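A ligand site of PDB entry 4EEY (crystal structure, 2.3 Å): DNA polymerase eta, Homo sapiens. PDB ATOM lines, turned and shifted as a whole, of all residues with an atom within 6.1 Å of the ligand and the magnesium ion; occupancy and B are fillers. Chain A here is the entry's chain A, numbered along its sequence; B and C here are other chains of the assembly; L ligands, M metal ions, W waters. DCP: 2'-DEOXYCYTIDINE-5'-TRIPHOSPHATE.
O6 of DG 5 of chain B is in hydrogen-bond range of a nitrogen (N4) of the ligand, at 3.2 Å.
An oxygen (O1G) of the ligand lies close to the side-chain amino group of Lys 234, at 3.6 Å.
The backbone NH (N) of Phe 20 sits at hydrogen-bond distance from an oxygen (O3') of the ligand, at 3.4 Å.
An oxygen (O3G) of the ligand sits at hydrogen-bond distance from the backbone NH of Cys 19.
An oxygen (O3G) of the ligand lies within hydrogen-bond range of the side-chain hydroxyl (OH) of Tyr 55 (2.8 Å).
The guanidinium group (NH2) of Arg 64 lies within salt-bridge range of an oxygen (O2B) of the ligand, at 3.4 Å.
N of Phe 21 is in hydrogen-bond range of O3' of the ligand (3.1 Å).
The guanidinium group (NH1) of Arg 58 is in salt-bridge range of an oxygen (O2G) of the ligand, 3.2 Å away.
N6 of DA 9 of chain C sits at hydrogen-bond distance from a nitrogen (N4) of the ligand, 3.4 Å away.
OH of Tyr 55 sits close to NH1 of Arg 58.
The backbone NH (N) of Asp 118 lies close to the side-chain hydroxyl (OG) of Ser 116, 3.3 Å away.
NZ of Lys 234 is in salt-bridge range of OD2 of Asp 16 (3.3 Å).
The guanidinium group (NE) of Arg 58 sits at hydrogen-bond distance from the backbone carbonyl oxygen (O) of Val 53, 2.8 Å away.
The side-chain carboxylate of Asp 16 lies within salt-bridge range of the side-chain amino group of Lys 227, at 3.7 Å.
The guanidinium group (NE) of Arg 64 sits at hydrogen-bond distance from the backbone carbonyl oxygen (O) of Ile 51 (2.8 Å).
OP2 of DA 9 of chain C lies within salt-bridge range of NZ of Lys 227 (3.0 Å).
CA of Asp 18 touches O3G of the ligand (3.3 Å).
O of Ile 51 touches C2' of the ligand, 3.5 Å away.
Ala 52 touches the ligand (CB to O3', 3.6 Å).
Ile 117 touches the ligand (CG2 to O4', 3.9 Å).
Within 4 Å of the ligand: Asp 16, Met 17, Asp 18, Cys 19, Phe 20, Phe 21, Ile 51, Ala 52, Tyr 55, Arg 58, Arg 64, Ile 117, Asp 118, Lys 234, DG 5 of chain B and DA 9 of chain C.
Of the 23 residues printed, 3 come within 4 Å of the magnesium ion.
The nearest printed residue that does not touch the magnesium ion is Asp 18 (4.4 Å).
The magnesium ion is bound by the backbone carbonyl oxygen (O) of Met 17 (2.2 Å), the side-chain carboxylate (OD1) of Asp 118 (2.2 Å), an oxygen (O1A) of the ligand (2.2 Å), an oxygen (O1G) of the ligand (2.2 Å), an oxygen (O1B) of the ligand (2.3 Å) and the side-chain carboxylate (OD1) of Asp 16 (2.3 Å).
The magnesium ion has six donor atoms within binding distance.
Water W4 bridges an oxygen (O2G) of the ligand and the guanidinium group (NH1) of Arg 58.
Water W1 lies within hydrogen-bond range of NZ of Lys 234 (2.6 Å), OD1 of Asp 18 (2.7 Å), O of Asp 16 (3.0 Å) and O3G of the ligand (3.5 Å).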
ATOM      1  N   ASP A  16     -16.189  -7.057  17.273  1.00  0.00           N
ATOM      2  CA  ASP A  16     -16.494  -8.197  18.139  1.00  0.00           C
ATOM      3  C   ASP A  16     -17.972  -8.215  18.549  1.00  0.00           C
ATOM      4  O   ASP A  16     -18.482  -7.258  19.140  1.00  0.00           O
ATOM      5  CB  ASP A  16     -15.563  -8.162  19.362  1.00  0.00           C
ATOM      6  CG  ASP A  16     -15.740  -9.356  20.284  1.00  0.00           C
ATOM      7  OD1 ASP A  16     -16.594 -10.225  20.026  1.00  0.00           O
ATOM      8  OD2 ASP A  16     -14.982  -9.430  21.272  1.00  0.00           O
ATOM      9  N   MET A  17     -18.643  -9.308  18.233  1.00  0.00           N
ATOM     10  CA  MET A  17     -20.073  -9.420  18.545  1.00  0.00           C
ATOM     11  C   MET A  17     -20.303  -9.492  20.052  1.00  0.00           C
ATOM     12  O   MET A  17     -19.563 -10.170  20.787  1.00  0.00           O
ATOM     13  CB  MET A  17     -20.697 -10.634  17.835  1.00  0.00           C
ATOM     14  CG  MET A  17     -20.347 -10.757  16.344  1.00  0.00           C
ATOM     15  SD  MET A  17     -20.698  -9.278  15.337  1.00  0.00           S
ATOM     16  CE  MET A  17     -22.470  -9.178  15.500  1.00  0.00           C
ATOM     17  N   ASP A  18     -21.315  -8.758  20.515  1.00  0.00           N
ATOM     18  CA  ASP A  18     -21.672  -8.732  21.927  1.00  0.00           C
ATOM     19  C   ASP A  18     -22.385 -10.040  22.260  1.00  0.00           C
ATOM     20  O   ASP A  18     -23.202 -10.519  21.468  1.00  0.00           O
ATOM     21  CB  ASP A  18     -22.576  -7.538  22.230  1.00  0.00           C
ATOM     22  CG  ASP A  18     -21.896  -6.190  22.018  1.00  0.00           C
ATOM     23  OD1 ASP A  18     -20.670  -6.083  22.234  1.00  0.00           O
ATOM     24  OD2 ASP A  18     -22.590  -5.218  21.647  1.00  0.00           O
ATOM     25  N   CYS A  19     -22.042 -10.617  23.413  1.00  0.00           N
ATOM     26  CA  CYS A  19     -22.647 -11.867  23.893  1.00  0.00           C
ATOM     27  C   CYS A  19     -23.209 -12.705  22.739  1.00  0.00           C
ATOM     28  O   CYS A  19     -24.416 -12.916  22.648  1.00  0.00           O
ATOM     29  CB  CYS A  19     -23.730 -11.568  24.932  1.00  0.00           C
ATOM     30  SG  CYS A  19     -25.030 -10.454  24.338  1.00  0.00           S
ATOM     31  N   PHE A  20     -22.310 -13.193  21.879  1.00  0.00           N
ATOM     32  CA  PHE A  20     -22.708 -13.664  20.552  1.00  0.00           C
ATOM     33  C   PHE A  20     -23.768 -14.766  20.498  1.00  0.00           C
ATOM     34  O   PHE A  20     -24.793 -14.590  19.841  1.00  0.00           O
ATOM     35  CB  PHE A  20     -21.489 -14.035  19.708  1.00  0.00           C
ATOM     36  CG  PHE A  20     -21.853 -14.450  18.305  1.00  0.00           C
ATOM     37  CD1 PHE A  20     -22.619 -13.612  17.507  1.00  0.00           C
ATOM     38  CD2 PHE A  20     -21.453 -15.678  17.800  1.00  0.00           C
ATOM     39  CE1 PHE A  20     -22.979 -13.989  16.212  1.00  0.00           C
ATOM     40  CE2 PHE A  20     -21.792 -16.058  16.510  1.00  0.00           C
ATOM     41  CZ  PHE A  20     -22.560 -15.211  15.710  1.00  0.00           C
ATOM     42  N   PHE A  21     -23.511 -15.894  21.157  1.00  0.00           N
ATOM     43  CA  PHE A  21     -24.450 -17.016  21.132  1.00  0.00           C
ATOM     44  C   PHE A  21     -25.807 -16.586  21.678  1.00  0.00           C
ATOM     45  O   PHE A  21     -26.837 -16.963  21.145  1.00  0.00           O
ATOM     46  CB  PHE A  21     -23.894 -18.243  21.881  1.00  0.00           C
ATOM     47  CG  PHE A  21     -22.764 -18.958  21.160  1.00  0.00           C
ATOM     48  CD1 PHE A  21     -22.016 -18.329  20.173  1.00  0.00           C
ATOM     49  CD2 PHE A  21     -22.424 -20.259  21.524  1.00  0.00           C
ATOM     50  CE1 PHE A  21     -20.959 -18.995  19.533  1.00  0.00           C
ATOM     51  CE2 PHE A  21     -21.365 -20.934  20.886  1.00  0.00           C
ATOM     52  CZ  PHE A  21     -20.640 -20.293  19.892  1.00  0.00           C
ATOM     53  N   VAL A  22     -25.792 -15.763  22.732  1.00  0.00           N
ATOM     54  CA  VAL A  22     -27.024 -15.173  23.287  1.00  0.00           C
ATOM     55  C   VAL A  22     -27.831 -14.386  22.240  1.00  0.00           C
ATOM     56  O   VAL A  22     -29.033 -14.637  22.064  1.00  0.00           O
ATOM     57  CB  VAL A  22     -26.712 -14.306  24.540  1.00  0.00           C
ATOM     58  CG1 VAL A  22     -27.904 -13.446  24.912  1.00  0.00           C
ATOM     59  CG2 VAL A  22     -26.313 -15.171  25.712  1.00  0.00           C
ATOM     60  N   ILE A  51     -22.429 -21.096  28.468  1.00  0.00           N
ATOM     61  CA  ILE A  51     -21.361 -20.754  27.524  1.00  0.00           C
ATOM     62  C   ILE A  51     -21.387 -19.305  27.003  1.00  0.00           C
ATOM     63  O   ILE A  51     -20.408 -18.855  26.405  1.00  0.00           O
ATOM     64  CB  ILE A  51     -21.233 -21.784  26.359  1.00  0.00           C
ATOM     65  CG1 ILE A  51     -22.520 -21.852  25.523  1.00  0.00           C
ATOM     66  CG2 ILE A  51     -20.840 -23.163  26.913  1.00  0.00           C
ATOM     67  CD1 ILE A  51     -22.379 -22.695  24.267  1.00  0.00           C
ATOM     68  N   ALA A  52     -22.503 -18.604  27.232  1.00  0.00           N
ATOM     69  CA  ALA A  52     -22.661 -17.188  26.886  1.00  0.00           C
ATOM     70  C   ALA A  52     -23.718 -16.538  27.778  1.00  0.00           C
ATOM     71  O   ALA A  52     -24.683 -17.190  28.185  1.00  0.00           O
ATOM     72  CB  ALA A  52     -23.040 -17.011  25.410  1.00  0.00           C
ATOM     73  N   VAL A  53     -23.520 -15.252  28.087  1.00  0.00           N
ATOM     74  CA  VAL A  53     -24.320 -14.566  29.109  1.00  0.00           C
ATOM     75  C   VAL A  53     -24.701 -13.164  28.636  1.00  0.00           C
ATOM     76  O   VAL A  53     -23.832 -12.381  28.280  1.00  0.00           O
ATOM     77  CB  VAL A  53     -23.512 -14.407  30.430  1.00  0.00           C
ATOM     78  CG1 VAL A  53     -24.428 -13.924  31.566  1.00  0.00           C
ATOM     79  CG2 VAL A  53     -22.803 -15.696  30.806  1.00  0.00           C
ATOM     80  N   TYR A  55     -25.783  -9.216  28.869  1.00  0.00           N
ATOM     81  CA  TYR A  55     -25.344  -8.127  29.748  1.00  0.00           C
ATOM     82  C   TYR A  55     -26.289  -7.888  30.940  1.00  0.00           C
ATOM     83  O   TYR A  55     -25.836  -7.602  32.042  1.00  0.00           O
ATOM     84  CB  TYR A  55     -25.053  -6.849  28.939  1.00  0.00           C
ATOM     85  CG  TYR A  55     -23.715  -6.947  28.230  1.00  0.00           C
ATOM     86  CD1 TYR A  55     -23.590  -7.645  27.018  1.00  0.00           C
ATOM     87  CD2 TYR A  55     -22.558  -6.394  28.790  1.00  0.00           C
ATOM     88  CE1 TYR A  55     -22.348  -7.768  26.375  1.00  0.00           C
ATOM     89  CE2 TYR A  55     -21.308  -6.514  28.149  1.00  0.00           C
ATOM     90  CZ  TYR A  55     -21.213  -7.195  26.959  1.00  0.00           C
ATOM     91  OH  TYR A  55     -19.986  -7.311  26.322  1.00  0.00           O
ATOM     92  N   ARG A  58     -25.193 -10.479  33.389  1.00  0.00           N
ATOM     93  CA  ARG A  58     -23.878 -10.172  33.972  1.00  0.00           C
ATOM     94  C   ARG A  58     -23.977  -9.249  35.193  1.00  0.00           C
ATOM     95  O   ARG A  58     -23.229  -9.414  36.174  1.00  0.00           O
ATOM     96  CB  ARG A  58     -22.929  -9.602  32.924  1.00  0.00           C
ATOM     97  CG  ARG A  58     -22.508 -10.622  31.859  1.00  0.00           C
ATOM     98  CD  ARG A  58     -21.705  -9.992  30.718  1.00  0.00           C
ATOM     99  NE  ARG A  58     -21.840 -10.758  29.474  1.00  0.00           N
ATOM    100  CZ  ARG A  58     -20.989 -10.708  28.451  1.00  0.00           C
ATOM    101  NH1 ARG A  58     -19.909  -9.928  28.481  1.00  0.00           N
ATOM    102  NH2 ARG A  58     -21.228 -11.427  27.364  1.00  0.00           N
ATOM    103  N   ARG A  64     -19.591 -17.173  32.439  1.00  0.00           N
ATOM    104  CA  ARG A  64     -19.366 -18.415  31.703  1.00  0.00           C
ATOM    105  C   ARG A  64     -18.845 -19.543  32.603  1.00  0.00           C
ATOM    106  O   ARG A  64     -18.007 -19.317  33.485  1.00  0.00           O
ATOM    107  CB  ARG A  64     -18.387 -18.185  30.542  1.00  0.00           C
ATOM    108  CG  ARG A  64     -18.104 -19.424  29.693  1.00  0.00           C
ATOM    109  CD  ARG A  64     -17.252 -19.134  28.454  1.00  0.00           C
ATOM    110  NE  ARG A  64     -17.942 -18.258  27.489  1.00  0.00           N
ATOM    111  CZ  ARG A  64     -17.585 -17.003  27.226  1.00  0.00           C
ATOM    112  NH1 ARG A  64     -16.539 -16.462  27.838  1.00  0.00           N
ATOM    113  NH2 ARG A  64     -18.279 -16.303  26.341  1.00  0.00           N
ATOM    114  N   SER A 116     -11.961 -15.453  14.971  1.00  0.00           N
ATOM    115  CA  SER A 116     -12.796 -16.385  15.743  1.00  0.00           C
ATOM    116  C   SER A 116     -14.210 -16.437  15.147  1.00  0.00           C
ATOM    117  O   SER A 116     -14.474 -15.804  14.125  1.00  0.00           O
ATOM    118  CB  SER A 116     -12.864 -15.923  17.203  1.00  0.00           C
ATOM    119  OG  SER A 116     -13.730 -14.799  17.340  1.00  0.00           O
ATOM    120  N   ILE A 117     -15.110 -17.168  15.809  1.00  0.00           N
ATOM    121  CA  ILE A 117     -16.520 -17.242  15.384  1.00  0.00           C
ATOM    122  C   ILE A 117     -17.197 -15.870  15.321  1.00  0.00           C
ATOM    123  O   ILE A 117     -18.058 -15.647  14.462  1.00  0.00           O
ATOM    124  CB  ILE A 117     -17.363 -18.227  16.266  1.00  0.00           C
ATOM    125  CG1 ILE A 117     -18.695 -18.589  15.565  1.00  0.00           C
ATOM    126  CG2 ILE A 117     -17.613 -17.683  17.675  1.00  0.00           C
ATOM    127  CD1 ILE A 117     -19.245 -19.960  15.963  1.00  0.00           C
ATOM    128  N   ASP A 118     -16.808 -14.946  16.207  1.00  0.00           N
ATOM    129  CA  ASP A 118     -17.533 -13.678  16.359  1.00  0.00           C
ATOM    130  C   ASP A 118     -16.655 -12.426  16.339  1.00  0.00           C
ATOM    131  O   ASP A 118     -17.060 -11.355  16.818  1.00  0.00           O
ATOM    132  CB  ASP A 118     -18.376 -13.708  17.639  1.00  0.00           C
ATOM    133  CG  ASP A 118     -17.578 -13.334  18.880  1.00  0.00           C
ATOM    134  OD1 ASP A 118     -18.109 -12.574  19.717  1.00  0.00           O
ATOM    135  OD2 ASP A 118     -16.410 -13.784  19.002  1.00  0.00           O
ATOM    136  N   GLU A 119     -15.434 -12.546  15.826  1.00  0.00           N
ATOM    137  CA  GLU A 119     -14.580 -11.385  15.682  1.00  0.00           C
ATOM    138  C   GLU A 119     -13.758 -11.455  14.415  1.00  0.00           C
ATOM    139  O   GLU A 119     -13.345 -12.534  13.980  1.00  0.00           O
ATOM    140  CB  GLU A 119     -13.706 -11.144  16.941  1.00  0.00           C
ATOM    141  CG  GLU A 119     -12.340 -11.804  16.954  1.00  0.00           C
ATOM    142  CD  GLU A 119     -11.782 -12.037  18.362  1.00  0.00           C
ATOM    143  OE1 GLU A 119     -11.724 -11.077  19.164  1.00  0.00           O
ATOM    144  OE2 GLU A 119     -11.375 -13.186  18.642  1.00  0.00           O
ATOM    145  N   LYS A 227      -7.765  -4.664  19.466  1.00  0.00           N
ATOM    146  CA  LYS A 227      -8.418  -5.659  20.317  1.00  0.00           C
ATOM    147  C   LYS A 227      -8.581  -5.127  21.746  1.00  0.00           C
ATOM    148  O   LYS A 227      -9.633  -5.316  22.357  1.00  0.00           O
ATOM    149  CB  LYS A 227      -7.621  -6.972  20.292  1.00  0.00           C
ATOM    150  CG  LYS A 227      -8.073  -8.051  21.292  1.00  0.00           C
ATOM    151  CD  LYS A 227      -9.449  -8.584  20.931  1.00  0.00           C
ATOM    152  CE  LYS A 227      -9.975  -9.519  22.006  1.00  0.00           C
ATOM    153  NZ  LYS A 227     -11.390  -9.889  21.744  1.00  0.00           N
ATOM    154  N   LYS A 234     -17.954  -1.694  26.204  1.00  0.00           N
ATOM    155  CA  LYS A 234     -18.933  -2.665  25.731  1.00  0.00           C
ATOM    156  C   LYS A 234     -20.172  -2.520  26.598  1.00  0.00           C
ATOM    157  O   LYS A 234     -20.084  -1.986  27.696  1.00  0.00           O
ATOM    158  CB  LYS A 234     -18.341  -4.069  25.865  1.00  0.00           C
ATOM    159  CG  LYS A 234     -17.295  -4.406  24.804  1.00  0.00           C
ATOM    160  CD  LYS A 234     -16.454  -5.583  25.251  1.00  0.00           C
ATOM    161  CE  LYS A 234     -16.982  -6.912  24.746  1.00  0.00           C
ATOM    162  NZ  LYS A 234     -16.229  -7.356  23.539  1.00  0.00           N
ATOM    163  N   PRO A 235     -21.346  -2.964  26.109  1.00  0.00           N
ATOM    164  CA  PRO A 235     -21.672  -3.449  24.767  1.00  0.00           C
ATOM    165  C   PRO A 235     -22.056  -2.323  23.813  1.00  0.00           C
ATOM    166  O   PRO A 235     -22.258  -1.199  24.242  1.00  0.00           O
ATOM    167  CB  PRO A 235     -22.895  -4.337  25.016  1.00  0.00           C
ATOM    168  CG  PRO A 235     -23.587  -3.667  26.146  1.00  0.00           C
ATOM    169  CD  PRO A 235     -22.486  -3.120  27.027  1.00  0.00           C
ATOM    170  P    DG B   5     -16.799 -31.486  30.916  1.00  0.00           P
ATOM    171  OP1  DG B   5     -17.662 -32.687  30.993  1.00  0.00           O
ATOM    172  OP2  DG B   5     -15.382 -31.629  30.500  1.00  0.00           O
ATOM    173  O5'  DG B   5     -17.447 -30.394  29.944  1.00  0.00           O
ATOM    174  C5'  DG B   5     -18.808 -30.337  29.600  1.00  0.00           C
ATOM    175  C4'  DG B   5     -18.876 -29.821  28.183  1.00  0.00           C
ATOM    176  O4'  DG B   5     -18.402 -28.444  28.141  1.00  0.00           O
ATOM    177  C3'  DG B   5     -18.018 -30.585  27.166  1.00  0.00           C
ATOM    178  O3'  DG B   5     -18.799 -30.764  25.998  1.00  0.00           O
ATOM    179  C2'  DG B   5     -16.823 -29.675  26.907  1.00  0.00           C
ATOM    180  C1'  DG B   5     -17.480 -28.306  27.077  1.00  0.00           C
ATOM    181  N9   DG B   5     -16.579 -27.194  27.386  1.00  0.00           N
ATOM    182  C8   DG B   5     -15.504 -27.144  28.252  1.00  0.00           C
ATOM    183  N7   DG B   5     -14.913 -25.987  28.303  1.00  0.00           N
ATOM    184  C5   DG B   5     -15.653 -25.216  27.418  1.00  0.00           C
ATOM    185  C6   DG B   5     -15.508 -23.853  27.030  1.00  0.00           C
ATOM    186  O6   DG B   5     -14.650 -23.055  27.435  1.00  0.00           O
ATOM    187  N1   DG B   5     -16.463 -23.452  26.090  1.00  0.00           N
ATOM    188  C2   DG B   5     -17.447 -24.272  25.580  1.00  0.00           C
ATOM    189  N2   DG B   5     -18.309 -23.757  24.682  1.00  0.00           N
ATOM    190  N3   DG B   5     -17.587 -25.545  25.933  1.00  0.00           N
ATOM    191  C4   DG B   5     -16.671 -25.943  26.843  1.00  0.00           C
ATOM    192  P    DT B   6     -18.378 -31.730  24.800  1.00  0.00           P
ATOM    193  OP1  DT B   6     -19.561 -32.569  24.521  1.00  0.00           O
ATOM    194  OP2  DT B   6     -17.068 -32.370  25.067  1.00  0.00           O
ATOM    195  O5'  DT B   6     -18.232 -30.698  23.599  1.00  0.00           O
ATOM    196  C5'  DT B   6     -19.392 -29.997  23.115  1.00  0.00           C
ATOM    197  C4'  DT B   6     -19.013 -29.047  21.986  1.00  0.00           C
ATOM    198  O4'  DT B   6     -18.269 -27.913  22.508  1.00  0.00           O
ATOM    199  C3'  DT B   6     -18.139 -29.640  20.892  1.00  0.00           C
ATOM    200  O3'  DT B   6     -18.519 -29.050  19.667  1.00  0.00           O
ATOM    201  C2'  DT B   6     -16.732 -29.230  21.332  1.00  0.00           C
ATOM    202  C1'  DT B   6     -17.034 -27.822  21.827  1.00  0.00           C
ATOM    203  N1   DT B   6     -16.017 -27.206  22.752  1.00  0.00           N
ATOM    204  C2   DT B   6     -15.812 -25.838  22.666  1.00  0.00           C
ATOM    205  O2   DT B   6     -16.415 -25.106  21.888  1.00  0.00           O
ATOM    206  N3   DT B   6     -14.872 -25.346  23.533  1.00  0.00           N
ATOM    207  C4   DT B   6     -14.153 -26.073  24.458  1.00  0.00           C
ATOM    208  O4   DT B   6     -13.334 -25.512  25.185  1.00  0.00           O
ATOM    209  C5   DT B   6     -14.403 -27.508  24.495  1.00  0.00           C
ATOM    210  C7   DT B   6     -13.665 -28.393  25.451  1.00  0.00           C
ATOM    211  C6   DT B   6     -15.325 -28.000  23.652  1.00  0.00           C
ATOM    212  P    DA C   9      -9.527 -13.891  21.786  1.00  0.00           P
ATOM    213  OP1  DA C   9      -8.353 -13.806  20.887  1.00  0.00           O
ATOM    214  OP2  DA C   9     -10.321 -12.678  22.026  1.00  0.00           O
ATOM    215  O5'  DA C   9     -10.529 -15.020  21.262  1.00  0.00           O
ATOM    216  C5'  DA C   9     -11.881 -15.019  21.716  1.00  0.00           C
ATOM    217  C4'  DA C   9     -12.747 -15.944  20.876  1.00  0.00           C
ATOM    218  O4'  DA C   9     -12.159 -17.273  20.789  1.00  0.00           O
ATOM    219  C3'  DA C   9     -14.152 -16.148  21.447  1.00  0.00           C
ATOM    220  C2'  DA C   9     -14.520 -17.548  20.976  1.00  0.00           C
ATOM    221  C1'  DA C   9     -13.172 -18.259  20.932  1.00  0.00           C
ATOM    222  N9   DA C   9     -12.874 -19.081  22.107  1.00  0.00           N
ATOM    223  C8   DA C   9     -12.044 -18.776  23.149  1.00  0.00           C
ATOM    224  N7   DA C   9     -11.955 -19.716  24.062  1.00  0.00           N
ATOM    225  C5   DA C   9     -12.796 -20.717  23.592  1.00  0.00           C
ATOM    226  C6   DA C   9     -13.141 -21.987  24.098  1.00  0.00           C
ATOM    227  N6   DA C   9     -12.672 -22.492  25.245  1.00  0.00           N
ATOM    228  N1   DA C   9     -14.002 -22.732  23.373  1.00  0.00           N
ATOM    229  C2   DA C   9     -14.480 -22.230  22.225  1.00  0.00           C
ATOM    230  N3   DA C   9     -14.219 -21.057  21.646  1.00  0.00           N
ATOM    231  C4   DA C   9     -13.360 -20.342  22.386  1.00  0.00           C
HETATM  232  N1  DCP L   1     -17.390 -19.153  23.500  1.00  0.00           N
HETATM  233  C2  DCP L   1     -17.403 -20.423  24.148  1.00  0.00           C
HETATM  234  N3  DCP L   1     -16.487 -20.691  25.109  1.00  0.00           N
HETATM  235  C4  DCP L   1     -15.560 -19.765  25.465  1.00  0.00           C
HETATM  236  C5  DCP L   1     -15.535 -18.514  24.854  1.00  0.00           C
HETATM  237  C6  DCP L   1     -16.471 -18.237  23.867  1.00  0.00           C
HETATM  238  O2  DCP L   1     -18.239 -21.290  23.832  1.00  0.00           O
HETATM  239  N4  DCP L   1     -14.641 -20.042  26.428  1.00  0.00           N
HETATM  240  C1' DCP L   1     -18.376 -18.831  22.454  1.00  0.00           C
HETATM  241  C2' DCP L   1     -19.670 -18.270  23.063  1.00  0.00           C
HETATM  242  C3' DCP L   1     -19.552 -16.773  22.823  1.00  0.00           C
HETATM  243  C4' DCP L   1     -18.727 -16.669  21.558  1.00  0.00           C
HETATM  244  O4' DCP L   1     -17.859 -17.814  21.602  1.00  0.00           O
HETATM  245  O3' DCP L   1     -20.814 -16.109  22.686  1.00  0.00           O
HETATM  246  C5' DCP L   1     -17.900 -15.409  21.505  1.00  0.00           C
HETATM  247  O5' DCP L   1     -17.016 -15.380  22.626  1.00  0.00           O
HETATM  248  PA  DCP L   1     -16.625 -13.999  23.353  1.00  0.00           P
HETATM  249  O1A DCP L   1     -16.583 -12.894  22.325  1.00  0.00           O
HETATM  250  O2A DCP L   1     -15.397 -14.282  24.194  1.00  0.00           O
HETATM  251  O3A DCP L   1     -17.818 -13.723  24.394  1.00  0.00           O
HETATM  252  PB  DCP L   1     -19.281 -13.136  24.063  1.00  0.00           P
HETATM  253  O1B DCP L   1     -19.436 -12.649  22.643  1.00  0.00           O
HETATM  254  O2B DCP L   1     -20.265 -14.169  24.562  1.00  0.00           O
HETATM  255  O3B DCP L   1     -19.333 -11.862  25.067  1.00  0.00           O
HETATM  256  PG  DCP L   1     -18.676 -10.411  24.771  1.00  0.00           P
HETATM  257  O1G DCP L   1     -17.809 -10.565  23.548  1.00  0.00           O
HETATM  258  O2G DCP L   1     -17.904 -10.133  26.054  1.00  0.00           O
HETATM  259  O3G DCP L   1     -19.881  -9.525  24.588  1.00  0.00           O
HETATM  260 MG    MG M   1     -17.919 -11.371  21.509  1.00  0.00          MG
HETATM  261  O   HOH W   1     -18.412  -7.554  22.125  1.00  0.00           O
HETATM  262  O   HOH W   2     -20.922 -14.435  27.100  1.00  0.00           O
HETATM  263  O   HOH W   3     -12.986 -18.002  27.243  1.00  0.00           O
HETATM  264  O   HOH W   4     -17.189 -11.815  27.762  1.00  0.00           O
HETATM  265  O   HOH W   5     -18.391 -22.800  21.510  1.00  0.00           O
HETATM  266  O   HOH W   6     -14.337 -12.618  20.156  1.00  0.00           O
